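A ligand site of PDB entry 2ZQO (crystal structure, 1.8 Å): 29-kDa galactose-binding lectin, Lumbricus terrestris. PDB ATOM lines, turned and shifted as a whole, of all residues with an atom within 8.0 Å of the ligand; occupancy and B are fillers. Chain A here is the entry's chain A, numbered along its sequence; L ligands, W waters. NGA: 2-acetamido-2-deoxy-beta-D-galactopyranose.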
ATOM      1  N   VAL A  14      24.566 -29.302  22.557  1.00  0.00           N
ATOM      2  CA  VAL A  14      23.672 -29.113  23.707  1.00  0.00           C
ATOM      3  C   VAL A  14      22.485 -28.230  23.373  1.00  0.00           C
ATOM      4  O   VAL A  14      22.524 -27.453  22.430  1.00  0.00           O
ATOM      5  CB  VAL A  14      24.418 -28.491  24.884  1.00  0.00           C
ATOM      6  CG1 VAL A  14      25.522 -29.427  25.338  1.00  0.00           C
ATOM      7  CG2 VAL A  14      24.950 -27.072  24.514  1.00  0.00           C
ATOM      8  N   LEU A  15      21.418 -28.351  24.166  1.00  0.00           N
ATOM      9  CA  LEU A  15      20.276 -27.428  24.031  1.00  0.00           C
ATOM     10  C   LEU A  15      20.691 -26.020  24.420  1.00  0.00           C
ATOM     11  O   LEU A  15      21.394 -25.825  25.421  1.00  0.00           O
ATOM     12  CB  LEU A  15      19.069 -27.878  24.826  1.00  0.00           C
ATOM     13  CG  LEU A  15      18.455 -29.241  24.498  1.00  0.00           C
ATOM     14  CD1 LEU A  15      16.986 -29.261  24.958  1.00  0.00           C
ATOM     15  CD2 LEU A  15      18.625 -29.693  23.083  1.00  0.00           C
ATOM     16  N   ASP A  16      20.247 -25.053  23.616  1.00  0.00           N
ATOM     17  CA  ASP A  16      20.801 -23.690  23.626  1.00  0.00           C
ATOM     18  C   ASP A  16      19.681 -22.707  23.310  1.00  0.00           C
ATOM     19  O   ASP A  16      18.964 -22.921  22.316  1.00  0.00           O
ATOM     20  CB  ASP A  16      21.909 -23.664  22.582  1.00  0.00           C
ATOM     21  CG  ASP A  16      22.539 -22.269  22.340  1.00  0.00           C
ATOM     22  OD1 ASP A  16      23.775 -22.147  22.473  1.00  0.00           O
ATOM     23  OD2 ASP A  16      21.812 -21.332  21.944  1.00  0.00           O
ATOM     24  N   ILE A  17      19.476 -21.662  24.137  1.00  0.00           N
ATOM     25  CA  ILE A  17      18.521 -20.640  23.740  1.00  0.00           C
ATOM     26  C   ILE A  17      19.190 -19.746  22.696  1.00  0.00           C
ATOM     27  O   ILE A  17      20.145 -19.039  23.023  1.00  0.00           O
ATOM     28  CB  ILE A  17      18.008 -19.806  24.934  1.00  0.00           C
ATOM     29  CG1 ILE A  17      17.264 -20.698  25.922  1.00  0.00           C
ATOM     30  CG2 ILE A  17      17.062 -18.690  24.437  1.00  0.00           C
ATOM     31  CD1 ILE A  17      16.979 -19.909  27.272  1.00  0.00           C
ATOM     32  N   GLU A  18      18.699 -19.810  21.451  1.00  0.00           N
ATOM     33  CA  GLU A  18      19.323 -19.178  20.288  1.00  0.00           C
ATOM     34  C   GLU A  18      19.617 -17.690  20.526  1.00  0.00           C
ATOM     35  O   GLU A  18      18.739 -16.910  20.969  1.00  0.00           O
ATOM     36  CB  GLU A  18      18.395 -19.378  19.074  1.00  0.00           C
ATOM     37  CG  GLU A  18      18.845 -18.772  17.757  1.00  0.00           C
ATOM     38  CD  GLU A  18      18.122 -19.427  16.606  1.00  0.00           C
ATOM     39  OE1 GLU A  18      18.814 -20.033  15.755  1.00  0.00           O
ATOM     40  OE2 GLU A  18      16.876 -19.359  16.569  1.00  0.00           O
ATOM     41  N   GLY A  19      20.891 -17.349  20.287  1.00  0.00           N
ATOM     42  CA  GLY A  19      21.440 -16.036  20.465  1.00  0.00           C
ATOM     43  C   GLY A  19      21.422 -15.474  21.877  1.00  0.00           C
ATOM     44  O   GLY A  19      21.504 -14.251  22.053  1.00  0.00           O
ATOM     45  N   GLN A  20      21.307 -16.356  22.871  1.00  0.00           N
ATOM     46  CA  GLN A  20      21.189 -15.914  24.264  1.00  0.00           C
ATOM     47  C   GLN A  20      20.049 -14.927  24.453  1.00  0.00           C
ATOM     48  O   GLN A  20      20.127 -14.040  25.307  1.00  0.00           O
ATOM     49  CB  GLN A  20      22.484 -15.242  24.738  1.00  0.00           C
ATOM     50  CG  GLN A  20      23.638 -16.117  24.897  1.00  0.00           C
ATOM     51  CD  GLN A  20      24.673 -15.496  25.827  1.00  0.00           C
ATOM     52  OE1 GLN A  20      25.267 -14.461  25.520  1.00  0.00           O
ATOM     53  NE2 GLN A  20      24.863 -16.120  26.995  1.00  0.00           N
ATOM     54  N   ASN A  21      18.972 -15.115  23.693  1.00  0.00           N
ATOM     55  CA  ASN A  21      17.891 -14.142  23.643  1.00  0.00           C
ATOM     56  C   ASN A  21      16.980 -14.406  24.839  1.00  0.00           C
ATOM     57  O   ASN A  21      16.478 -15.516  25.008  1.00  0.00           O
ATOM     58  CB  ASN A  21      17.184 -14.318  22.295  1.00  0.00           C
ATOM     59  CG  ASN A  21      16.103 -13.274  22.012  1.00  0.00           C
ATOM     60  OD1 ASN A  21      15.740 -12.429  22.856  1.00  0.00           O
ATOM     61  ND2 ASN A  21      15.539 -13.356  20.788  1.00  0.00           N
ATOM     62  N   LYS A  27      13.941 -19.389  20.011  1.00  0.00           N
ATOM     63  CA  LYS A  27      14.036 -20.809  19.677  1.00  0.00           C
ATOM     64  C   LYS A  27      15.042 -21.552  20.537  1.00  0.00           C
ATOM     65  O   LYS A  27      16.099 -21.037  20.831  1.00  0.00           O
ATOM     66  CB  LYS A  27      14.389 -21.012  18.212  1.00  0.00           C
ATOM     67  CG  LYS A  27      13.352 -20.405  17.247  1.00  0.00           C
ATOM     68  CD  LYS A  27      12.029 -21.208  17.222  1.00  0.00           C
ATOM     69  CE  LYS A  27      11.115 -20.557  16.148  1.00  0.00           C
ATOM     70  NZ  LYS A  27       9.935 -21.435  15.840  1.00  0.00           N
ATOM     71  N   ILE A  29      17.591 -24.457  20.302  1.00  0.00           N
ATOM     72  CA  ILE A  29      18.299 -25.110  19.184  1.00  0.00           C
ATOM     73  C   ILE A  29      19.429 -26.000  19.756  1.00  0.00           C
ATOM     74  O   ILE A  29      19.685 -25.974  20.966  1.00  0.00           O
ATOM     75  CB  ILE A  29      18.924 -23.996  18.293  1.00  0.00           C
ATOM     76  CG1 ILE A  29      19.813 -23.078  19.154  1.00  0.00           C
ATOM     77  CG2 ILE A  29      17.851 -23.206  17.487  1.00  0.00           C
ATOM     78  CD1 ILE A  29      20.797 -22.265  18.368  1.00  0.00           C
ATOM     79  N   THR A  30      20.091 -26.787  18.900  1.00  0.00           N
ATOM     80  CA  THR A  30      21.341 -27.417  19.289  1.00  0.00           C
ATOM     81  C   THR A  30      22.511 -26.477  18.984  1.00  0.00           C
ATOM     82  O   THR A  30      22.433 -25.635  18.060  1.00  0.00           O
ATOM     83  CB  THR A  30      21.577 -28.772  18.548  1.00  0.00           C
ATOM     84  OG1 THR A  30      21.622 -28.542  17.140  1.00  0.00           O
ATOM     85  CG2 THR A  30      20.449 -29.733  18.908  1.00  0.00           C
ATOM     86  N   TRP A  31      23.571 -26.576  19.787  1.00  0.00           N
ATOM     87  CA  TRP A  31      24.751 -25.716  19.586  1.00  0.00           C
ATOM     88  C   TRP A  31      25.949 -26.360  20.250  1.00  0.00           C
ATOM     89  O   TRP A  31      25.789 -27.154  21.194  1.00  0.00           O
ATOM     90  CB  TRP A  31      24.508 -24.309  20.192  1.00  0.00           C
ATOM     91  CG  TRP A  31      25.457 -23.280  19.612  1.00  0.00           C
ATOM     92  CD1 TRP A  31      26.539 -22.717  20.229  1.00  0.00           C
ATOM     93  CD2 TRP A  31      25.421 -22.719  18.288  1.00  0.00           C
ATOM     94  NE1 TRP A  31      27.193 -21.852  19.375  1.00  0.00           N
ATOM     95  CE2 TRP A  31      26.504 -21.821  18.186  1.00  0.00           C
ATOM     96  CE3 TRP A  31      24.578 -22.888  17.181  1.00  0.00           C
ATOM     97  CZ2 TRP A  31      26.787 -21.097  17.005  1.00  0.00           C
ATOM     98  CZ3 TRP A  31      24.837 -22.139  16.006  1.00  0.00           C
ATOM     99  CH2 TRP A  31      25.934 -21.262  15.947  1.00  0.00           C
ATOM    100  N   ASP A  32      27.162 -26.029  19.773  1.00  0.00           N
ATOM    101  CA  ASP A  32      28.364 -26.537  20.427  1.00  0.00           C
ATOM    102  C   ASP A  32      28.403 -26.056  21.861  1.00  0.00           C
ATOM    103  O   ASP A  32      28.092 -24.883  22.143  1.00  0.00           O
ATOM    104  CB  ASP A  32      29.609 -26.077  19.694  1.00  0.00           C
ATOM    105  CG  ASP A  32      29.805 -26.783  18.324  1.00  0.00           C
ATOM    106  OD1 ASP A  32      30.543 -26.223  17.506  1.00  0.00           O
ATOM    107  OD2 ASP A  32      29.232 -27.862  18.075  1.00  0.00           O
ATOM    108  N   GLN A  33      28.758 -26.963  22.770  1.00  0.00           N
ATOM    109  CA  GLN A  33      28.882 -26.639  24.186  1.00  0.00           C
ATOM    110  C   GLN A  33      29.879 -25.521  24.487  1.00  0.00           C
ATOM    111  O   GLN A  33      31.021 -25.542  24.001  1.00  0.00           O
ATOM    112  CB  GLN A  33      29.244 -27.891  24.982  1.00  0.00           C
ATOM    113  CG  GLN A  33      29.123 -27.716  26.513  1.00  0.00           C
ATOM    114  CD  GLN A  33      29.531 -28.949  27.253  1.00  0.00           C
ATOM    115  OE1 GLN A  33      30.270 -29.786  26.726  1.00  0.00           O
ATOM    116  NE2 GLN A  33      29.050 -29.091  28.483  1.00  0.00           N
ATOM    117  N   LYS A  34      29.419 -24.565  25.300  1.00  0.00           N
ATOM    118  CA  LYS A  34      30.246 -23.470  25.820  1.00  0.00           C
ATOM    119  C   LYS A  34      30.394 -23.621  27.338  1.00  0.00           C
ATOM    120  O   LYS A  34      29.518 -24.182  27.995  1.00  0.00           O
ATOM    121  CB  LYS A  34      29.612 -22.103  25.534  1.00  0.00           C
ATOM    122  CG  LYS A  34      29.372 -21.762  24.054  1.00  0.00           C
ATOM    123  CD  LYS A  34      28.618 -20.413  23.896  1.00  0.00           C
ATOM    124  CE  LYS A  34      27.124 -20.572  24.215  1.00  0.00           C
ATOM    125  NZ  LYS A  34      26.501 -19.347  24.769  1.00  0.00           N
ATOM    126  N   PRO A  37      30.687 -17.845  31.941  1.00  0.00           N
ATOM    127  CA  PRO A  37      29.499 -17.000  32.092  1.00  0.00           C
ATOM    128  C   PRO A  37      28.567 -16.992  30.861  1.00  0.00           C
ATOM    129  O   PRO A  37      27.337 -17.043  31.020  1.00  0.00           O
ATOM    130  CB  PRO A  37      30.088 -15.607  32.353  1.00  0.00           C
ATOM    131  CG  PRO A  37      31.435 -15.880  32.945  1.00  0.00           C
ATOM    132  CD  PRO A  37      31.926 -17.094  32.189  1.00  0.00           C
ATOM    133  N   THR A  38      29.151 -16.952  29.669  1.00  0.00           N
ATOM    134  CA  THR A  38      28.363 -16.894  28.432  1.00  0.00           C
ATOM    135  C   THR A  38      27.529 -18.166  28.160  1.00  0.00           C
ATOM    136  O   THR A  38      26.612 -18.144  27.327  1.00  0.00           O
ATOM    137  CB  THR A  38      29.246 -16.569  27.199  1.00  0.00           C
ATOM    138  OG1 THR A  38      30.115 -17.671  26.908  1.00  0.00           O
ATOM    139  CG2 THR A  38      30.083 -15.306  27.466  1.00  0.00           C
ATOM    140  N   ALA A  39      27.833 -19.239  28.885  1.00  0.00           N
ATOM    141  CA  ALA A  39      27.076 -20.473  28.786  1.00  0.00           C
ATOM    142  C   ALA A  39      25.687 -20.457  29.445  1.00  0.00           C
ATOM    143  O   ALA A  39      25.019 -21.492  29.492  1.00  0.00           O
ATOM    144  CB  ALA A  39      27.895 -21.633  29.327  1.00  0.00           C
ATOM    145  N   VAL A  40      25.250 -19.312  29.973  1.00  0.00           N
ATOM    146  CA  VAL A  40      23.994 -19.280  30.725  1.00  0.00           C
ATOM    147  C   VAL A  40      22.802 -19.753  29.879  1.00  0.00           C
ATOM    148  O   VAL A  40      21.908 -20.408  30.402  1.00  0.00           O
ATOM    149  CB  VAL A  40      23.709 -17.890  31.404  1.00  0.00           C
ATOM    150  CG1 VAL A  40      23.590 -16.785  30.371  1.00  0.00           C
ATOM    151  CG2 VAL A  40      22.457 -17.967  32.225  1.00  0.00           C
ATOM    152  N   ASN A  41      22.807 -19.435  28.589  1.00  0.00           N
ATOM    153  CA  ASN A  41      21.732 -19.876  27.674  1.00  0.00           C
ATOM    154  C   ASN A  41      21.821 -21.367  27.277  1.00  0.00           C
ATOM    155  O   ASN A  41      21.022 -21.829  26.478  1.00  0.00           O
ATOM    156  CB  ASN A  41      21.687 -19.035  26.394  1.00  0.00           C
ATOM    157  CG  ASN A  41      22.934 -19.221  25.536  1.00  0.00           C
ATOM    158  OD1 ASN A  41      24.062 -19.259  26.052  1.00  0.00           O
ATOM    159  ND2 ASN A  41      22.741 -19.354  24.231  1.00  0.00           N
ATOM    160  N   GLN A  42      22.782 -22.095  27.861  1.00  0.00           N
ATOM    161  CA  GLN A  42      22.874 -23.543  27.660  1.00  0.00           C
ATOM    162  C   GLN A  42      22.732 -24.260  28.995  1.00  0.00           C
ATOM    163  O   GLN A  42      22.935 -25.462  29.069  1.00  0.00           O
ATOM    164  CB  GLN A  42      24.215 -23.922  27.019  1.00  0.00           C
ATOM    165  CG  GLN A  42      24.545 -23.183  25.727  1.00  0.00           C
ATOM    166  CD  GLN A  42      25.816 -23.749  25.097  1.00  0.00           C
ATOM    167  OE1 GLN A  42      26.692 -24.261  25.802  1.00  0.00           O
ATOM    168  NE2 GLN A  42      25.894 -23.708  23.768  1.00  0.00           N
ATOM    169  N   ALA A 108      24.728 -27.561  13.667  1.00  0.00           N
ATOM    170  CA  ALA A 108      24.478 -26.577  14.728  1.00  0.00           C
ATOM    171  C   ALA A 108      23.301 -25.719  14.318  1.00  0.00           C
ATOM    172  O   ALA A 108      23.103 -25.457  13.122  1.00  0.00           O
ATOM    173  CB  ALA A 108      25.714 -25.722  14.955  1.00  0.00           C
ATOM    174  N   GLY A 109      22.499 -25.282  15.277  1.00  0.00           N
ATOM    175  CA  GLY A 109      21.354 -24.445  14.918  1.00  0.00           C
ATOM    176  C   GLY A 109      20.065 -25.216  14.686  1.00  0.00           C
ATOM    177  O   GLY A 109      19.020 -24.614  14.454  1.00  0.00           O
HETATM  178  C1  NGA L   1      25.144 -17.081  19.640  1.00  0.00           C
HETATM  179  C2  NGA L   1      25.057 -17.719  21.025  1.00  0.00           C
HETATM  180  C3  NGA L   1      25.119 -19.249  20.872  1.00  0.00           C
HETATM  181  C4  NGA L   1      23.998 -19.712  19.936  1.00  0.00           C
HETATM  182  C5  NGA L   1      24.114 -18.947  18.609  1.00  0.00           C
HETATM  183  C6  NGA L   1      23.055 -19.319  17.580  1.00  0.00           C
HETATM  184  C7  NGA L   1      26.161 -16.174  22.575  1.00  0.00           C
HETATM  185  C8  NGA L   1      27.298 -16.096  23.555  1.00  0.00           C
HETATM  186  N2  NGA L   1      26.172 -17.272  21.821  1.00  0.00           N
HETATM  187  O1  NGA L   1      24.986 -15.663  19.742  1.00  0.00           O
HETATM  188  O3  NGA L   1      25.016 -19.883  22.139  1.00  0.00           O
HETATM  189  O4  NGA L   1      22.737 -19.451  20.570  1.00  0.00           O
HETATM  190  O5  NGA L   1      24.032 -17.540  18.888  1.00  0.00           O
HETATM  191  O6  NGA L   1      23.354 -18.682  16.310  1.00  0.00           O
HETATM  192  O7  NGA L   1      25.325 -15.281  22.460  1.00  0.00           O
HETATM  193  O   HOH W   1      25.180 -17.884  14.543  1.00  0.00           O
HETATM  194  O   HOH W   2      26.791 -14.745  17.461  1.00  0.00           O
HETATM  195  O   HOH W   3      21.284 -19.441  14.799  1.00  0.00           O
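O of Ile 17 touches O4 of the ligand (3.6 Å). Glu 18 touches the ligand. Ile 29 touches the ligand (CD1 to C6, 3.8 Å). Trp 31 touches the ligand. Hydrophobic or aromatic side chains within 4 Å of the ligand: Ile 29 and Trp 31. Nine residues have an atom within 4 Å of the ligand: Asp 16, Ile 17, Glu 18, Gly 19, Gln 20, Ile 29, Trp 31, Lys 34 and Asn 41. The nearest printed residue that does not touch the ligand is Thr 38 (4.2 Å).
An oxygen (O4) of the ligand lies within hydrogen-bond range of the side-chain carboxylate (OD2) of Asp 16 (2.5 Å). The backbone NH (N) of Gly 19 sits at hydrogen-bond distance from an oxygen (O4) of the ligand (2.8 Å). The side-chain amino group of Lys 34 sits close to an oxygen (O3) of the ligand. OE1 of Gln 20 lies close to O7 of the ligand, 3.2 Å away. The side-chain amide nitrogen of Asn 41 sits at hydrogen-bond distance from an oxygen (O3) of the ligand.
Water W3 lies within hydrogen-bond range of O6 of the ligand and OE1 of Glu 18.
The side-chain carboxylate of Asp 16 is in hydrogen-bond range of the side-chain amide nitrogen of Asn 41 (3.2 Å). OD2 of Asp 16 lies within hydrogen-bond range of N of Glu 18. N of Asp 16 sits at hydrogen-bond distance from O of Ile 29, at 2.9 Å. The side-chain carboxylate (OD1) of Asp 16 is in hydrogen-bond range of the side-chain amide nitrogen (NE2) of Gln 42 (2.9 Å). The side-chain amino group (NZ) of Lys 34 is in hydrogen-bond range of the side-chain amide oxygen (OD1) of Asn 41. OE1 of Gln 42 sits at hydrogen-bond distance from N of Lys 34 (2.8 Å). O of Asn 41 is in hydrogen-bond range of N of Ile 17, at 2.8 Å. The backbone NH (N) of Val 14 is in hydrogen-bond range of the backbone carbonyl oxygen (O) of Trp 31 (2.8 Å).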
